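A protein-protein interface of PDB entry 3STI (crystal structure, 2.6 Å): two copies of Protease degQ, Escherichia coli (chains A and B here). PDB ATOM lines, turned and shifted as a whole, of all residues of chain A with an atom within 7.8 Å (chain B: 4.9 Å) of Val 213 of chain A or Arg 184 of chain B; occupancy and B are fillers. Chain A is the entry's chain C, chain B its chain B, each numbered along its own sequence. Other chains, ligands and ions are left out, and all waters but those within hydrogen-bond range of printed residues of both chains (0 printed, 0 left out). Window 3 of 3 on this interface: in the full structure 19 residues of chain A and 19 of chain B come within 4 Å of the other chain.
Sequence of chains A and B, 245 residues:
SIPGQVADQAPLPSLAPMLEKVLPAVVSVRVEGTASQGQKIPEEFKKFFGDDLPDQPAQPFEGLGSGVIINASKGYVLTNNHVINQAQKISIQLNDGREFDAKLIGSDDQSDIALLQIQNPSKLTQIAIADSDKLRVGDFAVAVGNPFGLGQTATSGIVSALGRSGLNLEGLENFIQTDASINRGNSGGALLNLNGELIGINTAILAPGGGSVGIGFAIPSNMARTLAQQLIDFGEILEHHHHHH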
ATOM      1  N   GLY A 166       7.051  25.167  20.423  1.00  0.00           N
ATOM      2  CA  GLY A 166       7.893  25.506  21.566  1.00  0.00           C
ATOM      3  C   GLY A 166       7.322  25.156  22.921  1.00  0.00           C
ATOM      4  O   GLY A 166       8.082  24.885  23.854  1.00  0.00           O
ATOM      5  N   THR A 178       9.229  34.239  20.008  1.00  0.00           N
ATOM      6  CA  THR A 178      10.350  35.085  19.596  1.00  0.00           C
ATOM      7  C   THR A 178      11.374  35.159  20.736  1.00  0.00           C
ATOM      8  O   THR A 178      10.998  35.041  21.904  1.00  0.00           O
ATOM      9  CB  THR A 178       9.836  36.483  19.125  1.00  0.00           C
ATOM     10  OG1 THR A 178      10.921  37.247  18.629  1.00  0.00           O
ATOM     11  CG2 THR A 178       9.110  37.263  20.203  1.00  0.00           C
ATOM     12  N   LEU A 206       2.860  34.219  29.348  1.00  0.00           N
ATOM     13  CA  LEU A 206       3.493  32.948  28.997  1.00  0.00           C
ATOM     14  C   LEU A 206       2.462  31.814  28.944  1.00  0.00           C
ATOM     15  O   LEU A 206       1.864  31.570  27.893  1.00  0.00           O
ATOM     16  CB  LEU A 206       4.624  32.615  29.991  1.00  0.00           C
ATOM     17  CG  LEU A 206       5.955  33.355  29.763  1.00  0.00           C
ATOM     18  CD1 LEU A 206       5.999  34.684  30.517  1.00  0.00           C
ATOM     19  CD2 LEU A 206       7.141  32.490  30.169  1.00  0.00           C
ATOM     20  N   SER A 212       8.998  28.831  28.308  1.00  0.00           N
ATOM     21  CA  SER A 212      10.252  28.922  29.047  1.00  0.00           C
ATOM     22  C   SER A 212      10.826  30.355  29.017  1.00  0.00           C
ATOM     23  O   SER A 212      10.326  31.206  28.272  1.00  0.00           O
ATOM     24  CB  SER A 212      11.268  27.923  28.500  1.00  0.00           C
ATOM     25  OG  SER A 212      11.084  26.640  29.074  1.00  0.00           O
ATOM     26  N   VAL A 213      11.856  30.620  29.853  1.00  0.00           N
ATOM     27  CA  VAL A 213      12.504  31.930  29.959  1.00  0.00           C
ATOM     28  C   VAL A 213      13.357  32.187  28.690  1.00  0.00           C
ATOM     29  O   VAL A 213      13.774  31.233  28.022  1.00  0.00           O
ATOM     30  CB  VAL A 213      13.311  32.077  31.286  1.00  0.00           C
ATOM     31  CG1 VAL A 213      14.626  31.288  31.263  1.00  0.00           C
ATOM     32  CG2 VAL A 213      13.549  33.545  31.634  1.00  0.00           C
ATOM     33  N   GLY A 214      13.550  33.467  28.360  1.00  0.00           N
ATOM     34  CA  GLY A 214      14.300  33.898  27.186  1.00  0.00           C
ATOM     35  C   GLY A 214      13.472  33.999  25.917  1.00  0.00           C
ATOM     36  O   GLY A 214      13.934  34.586  24.932  1.00  0.00           O
ATOM     37  N   ILE A 215      12.251  33.422  25.928  1.00  0.00           N
ATOM     38  CA  ILE A 215      11.331  33.405  24.789  1.00  0.00           C
ATOM     39  C   ILE A 215      10.086  34.237  25.091  1.00  0.00           C
ATOM     40  O   ILE A 215       9.539  34.182  26.198  1.00  0.00           O
ATOM     41  CB  ILE A 215      10.927  31.969  24.347  1.00  0.00           C
ATOM     42  CG1 ILE A 215      11.971  30.919  24.763  1.00  0.00           C
ATOM     43  CG2 ILE A 215      10.657  31.911  22.840  1.00  0.00           C
ATOM     44  CD1 ILE A 215      11.389  29.747  25.423  1.00  0.00           C
ATOM     45  N   GLY A 216       9.663  34.998  24.090  1.00  0.00           N
ATOM     46  CA  GLY A 216       8.490  35.853  24.153  1.00  0.00           C
ATOM     47  C   GLY A 216       7.384  35.416  23.208  1.00  0.00           C
ATOM     48  O   GLY A 216       7.653  34.849  22.147  1.00  0.00           O
ATOM     49  N   PHE A 217       6.137  35.713  23.590  1.00  0.00           N
ATOM     50  CA  PHE A 217       4.921  35.346  22.873  1.00  0.00           C
ATOM     51  C   PHE A 217       4.236  36.539  22.216  1.00  0.00           C
ATOM     52  O   PHE A 217       4.108  37.607  22.816  1.00  0.00           O
ATOM     53  CB  PHE A 217       3.933  34.686  23.842  1.00  0.00           C
ATOM     54  CG  PHE A 217       4.429  33.395  24.432  1.00  0.00           C
ATOM     55  CD1 PHE A 217       5.181  33.390  25.600  1.00  0.00           C
ATOM     56  CD2 PHE A 217       4.131  32.177  23.830  1.00  0.00           C
ATOM     57  CE1 PHE A 217       5.642  32.190  26.142  1.00  0.00           C
ATOM     58  CE2 PHE A 217       4.587  30.981  24.380  1.00  0.00           C
ATOM     59  CZ  PHE A 217       5.336  30.994  25.532  1.00  0.00           C
ATOM     60  N   GLY B  65      13.241  16.444  25.715  1.00  0.00           N
ATOM     61  CA  GLY B  65      14.398  17.228  25.323  1.00  0.00           C
ATOM     62  C   GLY B  65      14.659  17.040  23.848  1.00  0.00           C
ATOM     63  O   GLY B  65      13.864  16.393  23.158  1.00  0.00           O
ATOM     64  N   PRO B 147      11.609  19.865  20.560  1.00  0.00           N
ATOM     65  CA  PRO B 147      10.936  19.033  21.568  1.00  0.00           C
ATOM     66  C   PRO B 147       9.490  18.759  21.141  1.00  0.00           C
ATOM     67  O   PRO B 147       8.939  19.469  20.275  1.00  0.00           O
ATOM     68  CB  PRO B 147      11.008  19.881  22.837  1.00  0.00           C
ATOM     69  CG  PRO B 147      11.047  21.314  22.337  1.00  0.00           C
ATOM     70  CD  PRO B 147      11.522  21.304  20.900  1.00  0.00           C
ATOM     71  N   SER B 181      19.462  32.299  23.892  1.00  0.00           N
ATOM     72  CA  SER B 181      18.700  31.671  24.973  1.00  0.00           C
ATOM     73  C   SER B 181      18.739  30.143  24.922  1.00  0.00           C
ATOM     74  O   SER B 181      18.424  29.535  23.894  1.00  0.00           O
ATOM     75  CB  SER B 181      17.263  32.163  24.967  1.00  0.00           C
ATOM     76  OG  SER B 181      17.266  33.579  25.096  1.00  0.00           O
ATOM     77  N   ILE B 182      19.205  29.541  26.032  1.00  0.00           N
ATOM     78  CA  ILE B 182      19.288  28.095  26.225  1.00  0.00           C
ATOM     79  C   ILE B 182      18.238  27.761  27.274  1.00  0.00           C
ATOM     80  O   ILE B 182      18.357  28.172  28.427  1.00  0.00           O
ATOM     81  CB  ILE B 182      20.716  27.580  26.592  1.00  0.00           C
ATOM     82  CG1 ILE B 182      21.826  28.190  25.699  1.00  0.00           C
ATOM     83  CG2 ILE B 182      20.779  26.031  26.629  1.00  0.00           C
ATOM     84  CD1 ILE B 182      21.804  27.859  24.184  1.00  0.00           C
ATOM     85  N   ASN B 183      17.171  27.095  26.842  1.00  0.00           N
ATOM     86  CA  ASN B 183      16.056  26.735  27.704  1.00  0.00           C
ATOM     87  C   ASN B 183      15.669  25.272  27.450  1.00  0.00           C
ATOM     88  O   ASN B 183      16.284  24.612  26.598  1.00  0.00           O
ATOM     89  CB  ASN B 183      14.881  27.692  27.481  1.00  0.00           C
ATOM     90  CG  ASN B 183      14.553  27.937  26.032  1.00  0.00           C
ATOM     91  OD1 ASN B 183      14.137  27.042  25.295  1.00  0.00           O
ATOM     92  ND2 ASN B 183      14.749  29.161  25.585  1.00  0.00           N
ATOM     93  N   ARG B 184      14.653  24.769  28.179  1.00  0.00           N
ATOM     94  CA  ARG B 184      14.164  23.390  28.077  1.00  0.00           C
ATOM     95  C   ARG B 184      13.706  23.012  26.656  1.00  0.00           C
ATOM     96  O   ARG B 184      13.678  21.827  26.341  1.00  0.00           O
ATOM     97  CB  ARG B 184      13.041  23.138  29.086  1.00  0.00           C
ATOM     98  CG  ARG B 184      13.529  22.936  30.525  1.00  0.00           C
ATOM     99  CD  ARG B 184      13.081  24.068  31.424  1.00  0.00           C
ATOM    100  NE  ARG B 184      13.944  25.242  31.256  1.00  0.00           N
ATOM    101  CZ  ARG B 184      13.542  26.507  31.339  1.00  0.00           C
ATOM    102  NH1 ARG B 184      12.264  26.793  31.562  1.00  0.00           N
ATOM    103  NH2 ARG B 184      14.412  27.495  31.175  1.00  0.00           N
ATOM    104  N   GLY B 185      13.433  24.007  25.812  1.00  0.00           N
ATOM    105  CA  GLY B 185      13.016  23.828  24.421  1.00  0.00           C
ATOM    106  C   GLY B 185      14.117  23.590  23.393  1.00  0.00           C
ATOM    107  O   GLY B 185      13.816  23.271  22.241  1.00  0.00           O
ATOM    108  N   ASN B 186      15.393  23.768  23.766  1.00  0.00           N
ATOM    109  CA  ASN B 186      16.494  23.497  22.826  1.00  0.00           C
ATOM    110  C   ASN B 186      17.648  22.731  23.526  1.00  0.00           C
ATOM    111  O   ASN B 186      18.618  22.349  22.873  1.00  0.00           O
ATOM    112  CB  ASN B 186      16.992  24.771  22.127  1.00  0.00           C
ATOM    113  CG  ASN B 186      17.424  25.910  23.011  1.00  0.00           C
ATOM    114  OD1 ASN B 186      17.753  25.756  24.205  1.00  0.00           O
ATOM    115  ND2 ASN B 186      17.476  27.088  22.407  1.00  0.00           N
ATOM    116  N   SER B 187      17.506  22.486  24.843  1.00  0.00           N
ATOM    117  CA  SER B 187      18.451  21.733  25.663  1.00  0.00           C
ATOM    118  C   SER B 187      18.550  20.291  25.153  1.00  0.00           C
ATOM    119  O   SER B 187      17.550  19.564  25.128  1.00  0.00           O
ATOM    120  CB  SER B 187      18.017  21.763  27.123  1.00  0.00           C
ATOM    121  OG  SER B 187      19.040  21.248  27.956  1.00  0.00           O
ATOM    122  N   ALA B 204      20.843  23.222  29.642  1.00  0.00           N
ATOM    123  CA  ALA B 204      20.149  24.171  30.493  1.00  0.00           C
ATOM    124  C   ALA B 204      20.350  23.909  32.000  1.00  0.00           C
ATOM    125  O   ALA B 204      19.901  24.745  32.787  1.00  0.00           O
ATOM    126  CB  ALA B 204      18.663  24.172  30.152  1.00  0.00           C
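The backbone carbonyl oxygen (O) of Gly 214 of chain A is in hydrogen-bond range of the side-chain hydroxyl (OG) of Ser 181 of chain B.
ND2 of Asn 183 of chain B lies within hydrogen-bond range of O of Val 213 of chain A (3.3 Å).
The guanidinium group of Arg 184 of chain B sits at hydrogen-bond distance from the side-chain hydroxyl of Ser 212 of chain A (2.8 Å).
OD1 of Asn 186 of chain B lies within hydrogen-bond range of N of Asn 183 of chain B, at 3.0 Å.
OD1 of Asn 183 of chain B lies close to N of Gly 185 of chain B (3.2 Å).
O of Ser 181 of chain B lies within hydrogen-bond range of ND2 of Asn 186 of chain B.
Among the printed residues, pairs that only touch across the chains: Ser 212 of chain A with Asn 183 of chain B (3.8 Å), Val 213 of chain A with Arg 184 of chain B (3.8 Å) and Ile 215 of chain A with Asn 183 of chain B (3.4 Å).
Leu 206 of chain A touches none of the printed residues of chain B.
Of the printed residues of chain B, Gly 214 of chain A touches Ser 181 (3.5 Å).
Of the printed residues of chain B, Ile 215 of chain A touches Asn 183 (3.4 Å).
Of the printed residues of chain A, Asn 183 of chain B touches Ser 212 (3.8 Å), Val 213 (3.3 Å) and Ile 215 (3.4 Å).
Of chain A, only Ser 212 (2.8 Å) and Val 213 (3.8 Å) come within 4 Å of Arg 184 of chain B.
Ser 187 of chain B touches none of the printed residues of chain A.
The nearest residue of chain B that does not touch Val 213 of chain A is Ser 181 of chain B (4.7 Å).
The nearest printed residue of chain A that does not touch Arg 184 of chain B is Gly 166 of chain A (6.6 Å).
The nearest printed residue of chain A that does not touch Asn 183 of chain B is Gly 214 of chain A (5.0 Å).
Printed residues of chain A that touch a printed residue of chain B: Ser 212, Val 213, Gly 214 and Ile 215.
Along chain A the printed residues that touch a printed residue of chain B span positions 212 to 215.
Of the 10 printed residues of chain B, 3 touch a printed residue of chain A.
Printed residues of chain B that touch a printed residue of chain A: Ser 181, Asn 183 and Arg 184.
Among the printed residues, no Asp or Glu carboxylate lies within 4 Å of a Lys or Arg side-chain nitrogen of the other chain.
No position is printed for both chains.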
